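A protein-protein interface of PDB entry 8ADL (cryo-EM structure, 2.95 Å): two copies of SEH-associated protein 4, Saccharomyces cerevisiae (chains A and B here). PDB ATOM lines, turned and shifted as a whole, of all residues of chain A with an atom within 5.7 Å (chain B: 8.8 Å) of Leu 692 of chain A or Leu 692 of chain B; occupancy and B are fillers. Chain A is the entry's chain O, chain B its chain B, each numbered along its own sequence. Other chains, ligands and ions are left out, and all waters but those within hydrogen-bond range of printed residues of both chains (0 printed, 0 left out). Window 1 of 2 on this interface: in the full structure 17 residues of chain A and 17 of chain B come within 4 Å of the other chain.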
ATOM      1  N   GLU A 688     -15.422 -29.732   3.970  1.00  0.00           N
ATOM      2  CA  GLU A 688     -14.166 -29.786   4.709  1.00  0.00           C
ATOM      3  C   GLU A 688     -13.529 -28.407   4.837  1.00  0.00           C
ATOM      4  O   GLU A 688     -12.820 -28.137   5.819  1.00  0.00           O
ATOM      5  CB  GLU A 688     -13.226 -30.766   4.010  1.00  0.00           C
ATOM      6  CG  GLU A 688     -12.045 -31.232   4.820  1.00  0.00           C
ATOM      7  CD  GLU A 688     -11.261 -32.301   4.092  1.00  0.00           C
ATOM      8  OE1 GLU A 688     -11.610 -32.610   2.933  1.00  0.00           O
ATOM      9  OE2 GLU A 688     -10.313 -32.848   4.681  1.00  0.00           O
ATOM     10  N   ARG A 689     -13.782 -27.531   3.859  1.00  0.00           N
ATOM     11  CA  ARG A 689     -13.225 -26.183   3.869  1.00  0.00           C
ATOM     12  C   ARG A 689     -13.788 -25.385   5.037  1.00  0.00           C
ATOM     13  O   ARG A 689     -13.060 -24.638   5.703  1.00  0.00           O
ATOM     14  CB  ARG A 689     -13.510 -25.495   2.535  1.00  0.00           C
ATOM     15  CG  ARG A 689     -13.030 -24.060   2.438  1.00  0.00           C
ATOM     16  CD  ARG A 689     -13.457 -23.438   1.118  1.00  0.00           C
ATOM     17  NE  ARG A 689     -14.028 -22.109   1.290  1.00  0.00           N
ATOM     18  CZ  ARG A 689     -14.679 -21.446   0.343  1.00  0.00           C
ATOM     19  NH1 ARG A 689     -14.861 -21.962  -0.860  1.00  0.00           N
ATOM     20  NH2 ARG A 689     -15.159 -20.236   0.612  1.00  0.00           N
ATOM     21  N   LEU A 690     -15.087 -25.546   5.298  1.00  0.00           N
ATOM     22  CA  LEU A 690     -15.722 -24.895   6.436  1.00  0.00           C
ATOM     23  C   LEU A 690     -15.164 -25.415   7.753  1.00  0.00           C
ATOM     24  O   LEU A 690     -15.053 -24.653   8.717  1.00  0.00           O
ATOM     25  CB  LEU A 690     -17.235 -25.094   6.373  1.00  0.00           C
ATOM     26  CG  LEU A 690     -17.926 -24.416   5.188  1.00  0.00           C
ATOM     27  CD1 LEU A 690     -19.434 -24.552   5.296  1.00  0.00           C
ATOM     28  CD2 LEU A 690     -17.522 -22.952   5.090  1.00  0.00           C
ATOM     29  N   ARG A 691     -14.805 -26.701   7.816  1.00  0.00           N
ATOM     30  CA  ARG A 691     -14.182 -27.235   9.025  1.00  0.00           C
ATOM     31  C   ARG A 691     -12.787 -26.651   9.227  1.00  0.00           C
ATOM     32  O   ARG A 691     -12.378 -26.387  10.365  1.00  0.00           O
ATOM     33  CB  ARG A 691     -14.138 -28.760   8.967  1.00  0.00           C
ATOM     34  CG  ARG A 691     -15.505 -29.402   8.808  1.00  0.00           C
ATOM     35  CD  ARG A 691     -15.560 -30.775   9.455  1.00  0.00           C
ATOM     36  NE  ARG A 691     -15.453 -31.847   8.474  1.00  0.00           N
ATOM     37  CZ  ARG A 691     -15.301 -33.129   8.780  1.00  0.00           C
ATOM     38  NH1 ARG A 691     -15.235 -33.537  10.036  1.00  0.00           N
ATOM     39  NH2 ARG A 691     -15.213 -34.024   7.799  1.00  0.00           N
ATOM     40  N   LEU A 692     -12.037 -26.454   8.136  1.00  0.00           N
ATOM     41  CA  LEU A 692     -10.734 -25.798   8.246  1.00  0.00           C
ATOM     42  C   LEU A 692     -10.878 -24.353   8.710  1.00  0.00           C
ATOM     43  O   LEU A 692     -10.090 -23.867   9.536  1.00  0.00           O
ATOM     44  CB  LEU A 692     -10.019 -25.836   6.896  1.00  0.00           C
ATOM     45  CG  LEU A 692      -9.472 -27.144   6.337  1.00  0.00           C
ATOM     46  CD1 LEU A 692      -9.139 -26.992   4.870  1.00  0.00           C
ATOM     47  CD2 LEU A 692      -8.216 -27.477   7.098  1.00  0.00           C
ATOM     48  N   ILE A 693     -11.899 -23.660   8.203  1.00  0.00           N
ATOM     49  CA  ILE A 693     -12.187 -22.297   8.642  1.00  0.00           C
ATOM     50  C   ILE A 693     -12.597 -22.285  10.112  1.00  0.00           C
ATOM     51  O   ILE A 693     -12.224 -21.380  10.869  1.00  0.00           O
ATOM     52  CB  ILE A 693     -13.259 -21.677   7.725  1.00  0.00           C
ATOM     53  CG1 ILE A 693     -12.667 -21.441   6.338  1.00  0.00           C
ATOM     54  CG2 ILE A 693     -13.751 -20.344   8.258  1.00  0.00           C
ATOM     55  CD1 ILE A 693     -13.685 -21.395   5.237  1.00  0.00           C
ATOM     56  N   ALA A 694     -13.339 -23.310  10.546  1.00  0.00           N
ATOM     57  CA  ALA A 694     -13.724 -23.430  11.949  1.00  0.00           C
ATOM     58  C   ALA A 694     -12.515 -23.646  12.847  1.00  0.00           C
ATOM     59  O   ALA A 694     -12.455 -23.103  13.955  1.00  0.00           O
ATOM     60  CB  ALA A 694     -14.716 -24.578  12.122  1.00  0.00           C
ATOM     61  N   THR A 695     -11.552 -24.453  12.395  1.00  0.00           N
ATOM     62  CA  THR A 695     -10.319 -24.640  13.157  1.00  0.00           C
ATOM     63  C   THR A 695      -9.530 -23.338  13.258  1.00  0.00           C
ATOM     64  O   THR A 695      -9.002 -22.999  14.329  1.00  0.00           O
ATOM     65  CB  THR A 695      -9.466 -25.737  12.521  1.00  0.00           C
ATOM     66  OG1 THR A 695     -10.300 -26.851  12.180  1.00  0.00           O
ATOM     67  CG2 THR A 695      -8.389 -26.198  13.486  1.00  0.00           C
ATOM     68  N   ALA A 696      -9.454 -22.587  12.153  1.00  0.00           N
ATOM     69  CA  ALA A 696      -8.778 -21.292  12.178  1.00  0.00           C
ATOM     70  C   ALA A 696      -9.474 -20.317  13.125  1.00  0.00           C
ATOM     71  O   ALA A 696      -8.812 -19.552  13.834  1.00  0.00           O
ATOM     72  CB  ALA A 696      -8.702 -20.712  10.767  1.00  0.00           C
ATOM     73  N   ILE A 697     -10.810 -20.319  13.133  1.00  0.00           N
ATOM     74  CA  ILE A 697     -11.571 -19.464  14.043  1.00  0.00           C
ATOM     75  C   ILE A 697     -11.331 -19.875  15.491  1.00  0.00           C
ATOM     76  O   ILE A 697     -11.117 -19.025  16.367  1.00  0.00           O
ATOM     77  CB  ILE A 697     -13.068 -19.495  13.678  1.00  0.00           C
ATOM     78  CG1 ILE A 697     -13.321 -18.712  12.394  1.00  0.00           C
ATOM     79  CG2 ILE A 697     -13.925 -18.917  14.793  1.00  0.00           C
ATOM     80  CD1 ILE A 697     -14.594 -19.119  11.702  1.00  0.00           C
ATOM     81  N   MET A 719      -5.488 -14.579   4.502  1.00  0.00           N
ATOM     82  CA  MET A 719      -6.710 -15.297   4.160  1.00  0.00           C
ATOM     83  C   MET A 719      -7.876 -14.343   3.942  1.00  0.00           C
ATOM     84  O   MET A 719      -8.730 -14.590   3.085  1.00  0.00           O
ATOM     85  CB  MET A 719      -7.057 -16.322   5.232  1.00  0.00           C
ATOM     86  CG  MET A 719      -6.193 -17.557   5.183  1.00  0.00           C
ATOM     87  SD  MET A 719      -6.559 -18.469   3.677  1.00  0.00           S
ATOM     88  CE  MET A 719      -8.219 -19.024   4.007  1.00  0.00           C
ATOM     89  N   PHE A 732     -12.664 -13.354   9.145  1.00  0.00           N
ATOM     90  CA  PHE A 732     -11.215 -13.315   9.320  1.00  0.00           C
ATOM     91  C   PHE A 732     -10.723 -11.918   9.678  1.00  0.00           C
ATOM     92  O   PHE A 732      -9.753 -11.783  10.434  1.00  0.00           O
ATOM     93  CB  PHE A 732     -10.517 -13.819   8.058  1.00  0.00           C
ATOM     94  CG  PHE A 732     -10.457 -15.317   7.959  1.00  0.00           C
ATOM     95  CD1 PHE A 732     -10.460 -16.100   9.103  1.00  0.00           C
ATOM     96  CD2 PHE A 732     -10.393 -15.942   6.724  1.00  0.00           C
ATOM     97  CE1 PHE A 732     -10.406 -17.478   9.019  1.00  0.00           C
ATOM     98  CE2 PHE A 732     -10.339 -17.321   6.632  1.00  0.00           C
ATOM     99  CZ  PHE A 732     -10.344 -18.089   7.782  1.00  0.00           C
ATOM    100  N   LEU B 682       4.323 -24.239   4.640  1.00  0.00           N
ATOM    101  CA  LEU B 682       2.951 -24.380   4.169  1.00  0.00           C
ATOM    102  C   LEU B 682       2.307 -23.036   3.867  1.00  0.00           C
ATOM    103  O   LEU B 682       1.346 -22.983   3.091  1.00  0.00           O
ATOM    104  CB  LEU B 682       2.111 -25.146   5.191  1.00  0.00           C
ATOM    105  CG  LEU B 682       1.861 -26.609   4.829  1.00  0.00           C
ATOM    106  CD1 LEU B 682       0.934 -27.260   5.829  1.00  0.00           C
ATOM    107  CD2 LEU B 682       1.301 -26.725   3.422  1.00  0.00           C
ATOM    108  N   GLY B 683       2.805 -21.954   4.459  1.00  0.00           N
ATOM    109  CA  GLY B 683       2.428 -20.634   4.001  1.00  0.00           C
ATOM    110  C   GLY B 683       3.003 -20.342   2.629  1.00  0.00           C
ATOM    111  O   GLY B 683       4.055 -20.861   2.248  1.00  0.00           O
ATOM    112  N   SER B 684       2.287 -19.490   1.887  1.00  0.00           N
ATOM    113  CA  SER B 684       2.609 -19.126   0.500  1.00  0.00           C
ATOM    114  C   SER B 684       2.716 -20.362  -0.392  1.00  0.00           C
ATOM    115  O   SER B 684       3.620 -20.476  -1.223  1.00  0.00           O
ATOM    116  CB  SER B 684       3.883 -18.280   0.420  1.00  0.00           C
ATOM    117  OG  SER B 684       5.041 -19.095   0.502  1.00  0.00           O
ATOM    118  N   ALA B 685       1.790 -21.298  -0.213  1.00  0.00           N
ATOM    119  CA  ALA B 685       1.723 -22.491  -1.039  1.00  0.00           C
ATOM    120  C   ALA B 685       0.845 -22.214  -2.259  1.00  0.00           C
ATOM    121  O   ALA B 685       0.456 -21.075  -2.526  1.00  0.00           O
ATOM    122  CB  ALA B 685       1.211 -23.675  -0.220  1.00  0.00           C
ATOM    123  N   LYS B 687      -2.129 -23.886  -2.842  1.00  0.00           N
ATOM    124  CA  LYS B 687      -3.493 -24.336  -2.595  1.00  0.00           C
ATOM    125  C   LYS B 687      -4.126 -23.573  -1.441  1.00  0.00           C
ATOM    126  O   LYS B 687      -3.468 -23.267  -0.443  1.00  0.00           O
ATOM    127  CB  LYS B 687      -3.537 -25.841  -2.308  1.00  0.00           C
ATOM    128  CG  LYS B 687      -3.354 -26.707  -3.544  1.00  0.00           C
ATOM    129  CD  LYS B 687      -4.004 -28.070  -3.366  1.00  0.00           C
ATOM    130  CE  LYS B 687      -3.177 -28.966  -2.460  1.00  0.00           C
ATOM    131  NZ  LYS B 687      -3.666 -30.373  -2.480  1.00  0.00           N
ATOM    132  N   GLU B 688      -5.416 -23.268  -1.599  1.00  0.00           N
ATOM    133  CA  GLU B 688      -6.192 -22.607  -0.553  1.00  0.00           C
ATOM    134  C   GLU B 688      -6.394 -23.511   0.659  1.00  0.00           C
ATOM    135  O   GLU B 688      -6.362 -23.044   1.808  1.00  0.00           O
ATOM    136  CB  GLU B 688      -7.541 -22.198  -1.137  1.00  0.00           C
ATOM    137  CG  GLU B 688      -8.465 -21.451  -0.218  1.00  0.00           C
ATOM    138  CD  GLU B 688      -9.848 -21.330  -0.821  1.00  0.00           C
ATOM    139  OE1 GLU B 688     -10.036 -21.781  -1.971  1.00  0.00           O
ATOM    140  OE2 GLU B 688     -10.756 -20.824  -0.140  1.00  0.00           O
ATOM    141  N   ARG B 689      -6.590 -24.809   0.414  1.00  0.00           N
ATOM    142  CA  ARG B 689      -6.708 -25.783   1.496  1.00  0.00           C
ATOM    143  C   ARG B 689      -5.416 -25.864   2.295  1.00  0.00           C
ATOM    144  O   ARG B 689      -5.441 -25.956   3.530  1.00  0.00           O
ATOM    145  CB  ARG B 689      -7.100 -27.146   0.925  1.00  0.00           C
ATOM    146  CG  ARG B 689      -7.200 -28.261   1.950  1.00  0.00           C
ATOM    147  CD  ARG B 689      -7.342 -29.615   1.278  1.00  0.00           C
ATOM    148  NE  ARG B 689      -6.545 -30.645   1.932  1.00  0.00           N
ATOM    149  CZ  ARG B 689      -6.304 -31.842   1.416  1.00  0.00           C
ATOM    150  NH1 ARG B 689      -6.781 -32.193   0.233  1.00  0.00           N
ATOM    151  NH2 ARG B 689      -5.566 -32.709   2.104  1.00  0.00           N
ATOM    152  N   LEU B 690      -4.277 -25.810   1.603  1.00  0.00           N
ATOM    153  CA  LEU B 690      -2.984 -25.802   2.274  1.00  0.00           C
ATOM    154  C   LEU B 690      -2.808 -24.545   3.117  1.00  0.00           C
ATOM    155  O   LEU B 690      -2.197 -24.596   4.187  1.00  0.00           O
ATOM    156  CB  LEU B 690      -1.860 -25.929   1.248  1.00  0.00           C
ATOM    157  CG  LEU B 690      -1.650 -27.332   0.674  1.00  0.00           C
ATOM    158  CD1 LEU B 690      -0.395 -27.387  -0.185  1.00  0.00           C
ATOM    159  CD2 LEU B 690      -1.607 -28.380   1.776  1.00  0.00           C
ATOM    160  N   ARG B 691      -3.339 -23.409   2.657  1.00  0.00           N
ATOM    161  CA  ARG B 691      -3.239 -22.181   3.444  1.00  0.00           C
ATOM    162  C   ARG B 691      -4.112 -22.255   4.694  1.00  0.00           C
ATOM    163  O   ARG B 691      -3.720 -21.763   5.761  1.00  0.00           O
ATOM    164  CB  ARG B 691      -3.608 -20.978   2.579  1.00  0.00           C
ATOM    165  CG  ARG B 691      -2.564 -20.676   1.517  1.00  0.00           C
ATOM    166  CD  ARG B 691      -2.620 -19.235   1.042  1.00  0.00           C
ATOM    167  NE  ARG B 691      -3.426 -19.088  -0.164  1.00  0.00           N
ATOM    168  CZ  ARG B 691      -3.730 -17.925  -0.724  1.00  0.00           C
ATOM    169  NH1 ARG B 691      -3.311 -16.781  -0.210  1.00  0.00           N
ATOM    170  NH2 ARG B 691      -4.473 -17.911  -1.827  1.00  0.00           N
ATOM    171  N   LEU B 692      -5.294 -22.873   4.587  1.00  0.00           N
ATOM    172  CA  LEU B 692      -6.126 -23.089   5.771  1.00  0.00           C
ATOM    173  C   LEU B 692      -5.449 -24.026   6.765  1.00  0.00           C
ATOM    174  O   LEU B 692      -5.493 -23.799   7.984  1.00  0.00           O
ATOM    175  CB  LEU B 692      -7.488 -23.646   5.361  1.00  0.00           C
ATOM    176  CG  LEU B 692      -8.512 -22.660   4.821  1.00  0.00           C
ATOM    177  CD1 LEU B 692      -9.665 -23.368   4.143  1.00  0.00           C
ATOM    178  CD2 LEU B 692      -9.026 -21.910   6.028  1.00  0.00           C
ATOM    179  N   ILE B 693      -4.804 -25.077   6.256  1.00  0.00           N
ATOM    180  CA  ILE B 693      -4.052 -25.995   7.109  1.00  0.00           C
ATOM    181  C   ILE B 693      -2.876 -25.275   7.761  1.00  0.00           C
ATOM    182  O   ILE B 693      -2.564 -25.502   8.937  1.00  0.00           O
ATOM    183  CB  ILE B 693      -3.611 -27.207   6.268  1.00  0.00           C
ATOM    184  CG1 ILE B 693      -4.830 -28.065   5.950  1.00  0.00           C
ATOM    185  CG2 ILE B 693      -2.585 -28.054   6.994  1.00  0.00           C
ATOM    186  CD1 ILE B 693      -4.667 -28.940   4.757  1.00  0.00           C
ATOM    187  N   ALA B 694      -2.241 -24.359   7.024  1.00  0.00           N
ATOM    188  CA  ALA B 694      -1.142 -23.569   7.569  1.00  0.00           C
ATOM    189  C   ALA B 694      -1.613 -22.658   8.694  1.00  0.00           C
ATOM    190  O   ALA B 694      -0.917 -22.499   9.701  1.00  0.00           O
ATOM    191  CB  ALA B 694      -0.485 -22.749   6.458  1.00  0.00           C
ATOM    192  N   THR B 695      -2.792 -22.049   8.537  1.00  0.00           N
ATOM    193  CA  THR B 695      -3.357 -21.235   9.612  1.00  0.00           C
ATOM    194  C   THR B 695      -3.688 -22.082  10.839  1.00  0.00           C
ATOM    195  O   THR B 695      -3.458 -21.657  11.981  1.00  0.00           O
ATOM    196  CB  THR B 695      -4.604 -20.503   9.115  1.00  0.00           C
ATOM    197  OG1 THR B 695      -4.328 -19.892   7.848  1.00  0.00           O
ATOM    198  CG2 THR B 695      -5.028 -19.430  10.104  1.00  0.00           C
ATOM    199  N   ALA B 696      -4.213 -23.292  10.617  1.00  0.00           N
ATOM    200  CA  ALA B 696      -4.505 -24.187  11.736  1.00  0.00           C
ATOM    201  C   ALA B 696      -3.235 -24.580  12.489  1.00  0.00           C
ATOM    202  O   ALA B 696      -3.231 -24.638  13.724  1.00  0.00           O
ATOM    203  CB  ALA B 696      -5.240 -25.429  11.235  1.00  0.00           C
ATOM    204  N   ILE B 697      -2.155 -24.870  11.759  1.00  0.00           N
ATOM    205  CA  ILE B 697      -0.886 -25.219  12.398  1.00  0.00           C
ATOM    206  C   ILE B 697      -0.281 -24.008  13.105  1.00  0.00           C
ATOM    207  O   ILE B 697       0.274 -24.124  14.205  1.00  0.00           O
ATOM    208  CB  ILE B 697       0.082 -25.801  11.351  1.00  0.00           C
ATOM    209  CG1 ILE B 697      -0.478 -27.091  10.767  1.00  0.00           C
ATOM    210  CG2 ILE B 697       1.454 -26.080  11.952  1.00  0.00           C
ATOM    211  CD1 ILE B 697       0.139 -27.443   9.439  1.00  0.00           C
ATOM    212  N   ALA B 698      -0.416 -22.822  12.503  1.00  0.00           N
ATOM    213  CA  ALA B 698       0.015 -21.574  13.126  1.00  0.00           C
ATOM    214  C   ALA B 698      -0.760 -21.239  14.391  1.00  0.00           C
ATOM    215  O   ALA B 698      -0.253 -20.489  15.231  1.00  0.00           O
ATOM    216  CB  ALA B 698      -0.110 -20.423  12.127  1.00  0.00           C
ATOM    217  N   GLY B 699      -1.964 -21.778  14.554  1.00  0.00           N
ATOM    218  CA  GLY B 699      -2.661 -21.616  15.821  1.00  0.00           C
ATOM    219  C   GLY B 699      -2.208 -22.517  16.955  1.00  0.00           C
ATOM    220  O   GLY B 699      -3.012 -22.875  17.821  1.00  0.00           O
ATOM    221  N   TRP B 712     -10.708 -26.290  20.624  1.00  0.00           N
ATOM    222  CA  TRP B 712      -9.783 -26.278  19.496  1.00  0.00           C
ATOM    223  C   TRP B 712      -8.960 -27.561  19.426  1.00  0.00           C
ATOM    224  O   TRP B 712      -8.686 -28.066  18.330  1.00  0.00           O
ATOM    225  CB  TRP B 712      -8.877 -25.052  19.597  1.00  0.00           C
ATOM    226  CG  TRP B 712      -7.834 -24.972  18.538  1.00  0.00           C
ATOM    227  CD1 TRP B 712      -7.946 -24.381  17.314  1.00  0.00           C
ATOM    228  CD2 TRP B 712      -6.499 -25.476  18.620  1.00  0.00           C
ATOM    229  NE1 TRP B 712      -6.766 -24.501  16.622  1.00  0.00           N
ATOM    230  CE2 TRP B 712      -5.861 -25.169  17.404  1.00  0.00           C
ATOM    231  CE3 TRP B 712      -5.783 -26.166  19.602  1.00  0.00           C
ATOM    232  CZ2 TRP B 712      -4.545 -25.529  17.144  1.00  0.00           C
ATOM    233  CZ3 TRP B 712      -4.478 -26.520  19.342  1.00  0.00           C
ATOM    234  CH2 TRP B 712      -3.871 -26.198  18.126  1.00  0.00           C
ATOM    235  N   GLN B 715     -11.229 -30.044  17.978  1.00  0.00           N
ATOM    236  CA  GLN B 715     -11.333 -29.824  16.539  1.00  0.00           C
ATOM    237  C   GLN B 715     -10.126 -30.389  15.804  1.00  0.00           C
ATOM    238  O   GLN B 715     -10.272 -31.010  14.746  1.00  0.00           O
ATOM    239  CB  GLN B 715     -11.479 -28.330  16.246  1.00  0.00           C
ATOM    240  CG  GLN B 715     -12.913 -27.837  16.185  1.00  0.00           C
ATOM    241  CD  GLN B 715     -13.680 -28.430  15.021  1.00  0.00           C
ATOM    242  OE1 GLN B 715     -13.211 -28.415  13.883  1.00  0.00           O
ATOM    243  NE2 GLN B 715     -14.866 -28.956  15.301  1.00  0.00           N
ATOM    244  N   MET B 719     -10.194 -33.406  13.130  1.00  0.00           N
ATOM    245  CA  MET B 719      -9.625 -33.165  11.809  1.00  0.00           C
ATOM    246  C   MET B 719      -8.535 -34.176  11.477  1.00  0.00           C
ATOM    247  O   MET B 719      -8.418 -34.613  10.326  1.00  0.00           O
ATOM    248  CB  MET B 719      -9.110 -31.735  11.720  1.00  0.00           C
ATOM    249  CG  MET B 719     -10.254 -30.772  11.503  1.00  0.00           C
ATOM    250  SD  MET B 719     -10.980 -30.921   9.871  1.00  0.00           S
ATOM    251  CE  MET B 719     -10.483 -29.373   9.166  1.00  0.00           C
ATOM    252  N   GLU B 722     -10.369 -37.340  10.520  1.00  0.00           N
ATOM    253  CA  GLU B 722     -11.141 -37.355   9.281  1.00  0.00           C
ATOM    254  C   GLU B 722     -10.298 -37.145   8.026  1.00  0.00           C
ATOM    255  O   GLU B 722     -10.776 -37.452   6.928  1.00  0.00           O
ATOM    256  CB  GLU B 722     -12.248 -36.289   9.317  1.00  0.00           C
ATOM    257  CG  GLU B 722     -11.774 -34.839   9.300  1.00  0.00           C
ATOM    258  CD  GLU B 722     -11.744 -34.250   7.894  1.00  0.00           C
ATOM    259  OE1 GLU B 722     -12.420 -34.809   7.004  1.00  0.00           O
ATOM    260  OE2 GLU B 722     -11.034 -33.250   7.673  1.00  0.00           O
ATOM    261  N   LEU B 723      -9.079 -36.627   8.149  1.00  0.00           N
ATOM    262  CA  LEU B 723      -8.290 -36.289   6.969  1.00  0.00           C
ATOM    263  C   LEU B 723      -7.743 -37.533   6.280  1.00  0.00           C
ATOM    264  O   LEU B 723      -7.461 -38.554   6.913  1.00  0.00           O
ATOM    265  CB  LEU B 723      -7.117 -35.388   7.360  1.00  0.00           C
ATOM    266  CG  LEU B 723      -7.225 -33.868   7.310  1.00  0.00           C
ATOM    267  CD1 LEU B 723      -5.971 -33.268   7.891  1.00  0.00           C
ATOM    268  CD2 LEU B 723      -7.373 -33.421   5.881  1.00  0.00           C
ATOM    269  N   LEU B 728      -0.693 -34.509   6.789  1.00  0.00           N
ATOM    270  CA  LEU B 728      -1.511 -33.543   7.512  1.00  0.00           C
ATOM    271  C   LEU B 728      -2.197 -34.179   8.716  1.00  0.00           C
ATOM    272  O   LEU B 728      -2.402 -33.509   9.737  1.00  0.00           O
ATOM    273  CB  LEU B 728      -2.533 -32.936   6.558  1.00  0.00           C
ATOM    274  CG  LEU B 728      -1.892 -32.490   5.244  1.00  0.00           C
ATOM    275  CD1 LEU B 728      -2.946 -32.066   4.255  1.00  0.00           C
ATOM    276  CD2 LEU B 728      -0.909 -31.358   5.492  1.00  0.00           C
ATOM    277  N   PHE B 732      -1.822 -32.704  12.499  1.00  0.00           N
ATOM    278  CA  PHE B 732      -2.947 -32.358  13.360  1.00  0.00           C
ATOM    279  C   PHE B 732      -3.039 -33.280  14.570  1.00  0.00           C
ATOM    280  O   PHE B 732      -3.530 -32.862  15.624  1.00  0.00           O
ATOM    281  CB  PHE B 732      -4.251 -32.381  12.567  1.00  0.00           C
ATOM    282  CG  PHE B 732      -4.469 -31.153  11.733  1.00  0.00           C
ATOM    283  CD1 PHE B 732      -3.745 -29.996  11.972  1.00  0.00           C
ATOM    284  CD2 PHE B 732      -5.410 -31.150  10.720  1.00  0.00           C
ATOM    285  CE1 PHE B 732      -3.944 -28.868  11.204  1.00  0.00           C
ATOM    286  CE2 PHE B 732      -5.616 -30.024   9.950  1.00  0.00           C
ATOM    287  CZ  PHE B 732      -4.883 -28.882  10.193  1.00  0.00           C
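Of the printed residues of chain B, Arg 689 of chain A touches Glu 688 (3.8 Å) and Leu 692 (3.8 Å).
Of chain B, only Arg 689 (3.7 Å), Leu 692 (3.7 Å), Ile 693 (3.6 Å) and Met 719 (3.5 Å) come within 4 Å of Leu 692 of chain A.
Ile 697 of chain A touches none of the printed residues of chain B.
Printed residues of chain A within 4 Å of Glu 688 of chain B: Arg 689.
Of chain A, only Arg 689, Leu 692, Ile 693 and Met 719 come within 4 Å of Leu 692 of chain B.
Arg 689 of chain A touches Leu 692 of chain B, and with the chains exchanged Leu 692 of chain A touches Arg 689 of chain B.
Arg 691 of chain A touches Met 719 of chain B, but with the chains exchanged Met 719 of chain A does not touch Arg 691 of chain B (4.03 Å).
Leu 692 of chain B touches its own counterpart, Leu 692 of chain A.
Thr 695 of chain A touches Met 719 of chain B, but with the chains exchanged Met 719 of chain A does not touch Thr 695 of chain B (4.004 Å).
Positions printed for both chains: 688, 689, 690, 691, 692, 693, 694, 695, 696, 697, 719 and 732.
Of the 17 pairs that touch across the chains among the printed residues, 9 have their exchanged pair printed and touching as well.
OE2 of Glu 688 of chain B is in salt-bridge range of NE of Arg 689 of chain A, at 3.8 Å.
The side-chain carboxylate (OE1) of Glu 722 of chain B is in salt-bridge range of the guanidinium group (NH2) of Arg 691 of chain A (3.0 Å).
OE2 of Glu 722 of chain B sits close to OE2 of Glu 688 of chain A.
Hydrophobic or aromatic side chains of chain B within 4 Å of the printed part of chain A: Leu 692, Ile 693, Ala 696, Trp 712, Met 719 and Leu 723.
Among the printed residues, 17 pairs touch across the chains.
Among the printed residues, merely in contact across the chains: Glu 688 of chain A with Leu 723 of chain B, Thr 695 of chain A with Trp 712 of chain B, Leu 692 of chain A with Met 719 of chain B, Arg 691 of chain A with Met 719 of chain B, Met 719 of chain A with Leu 692 of chain B, Leu 692 of chain A with Ile 693 of chain B, Leu 692 of chain A with Leu 692 of chain B, Ile 693 of chain A with Leu 692 of chain B, Thr 695 of chain A with Gln 715 of chain B, Leu 692 of chain A with Arg 689 of chain B, Arg 689 of chain A with Leu 692 of chain B, Thr 695 of chain A with Met 719 of chain B, Thr 695 of chain A with Ala 696 of chain B and Ala 696 of chain A with Thr 695 of chain B.
The backbone carbonyl oxygen (O) of Arg 691 of chain B sits at hydrogen-bond distance from the side-chain hydroxyl (OG1) of Thr 695 of chain B, at 2.9 Å.
OG1 of Thr 695 of chain A is in hydrogen-bond range of O of Arg 691 of chain A, at 2.8 Å.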
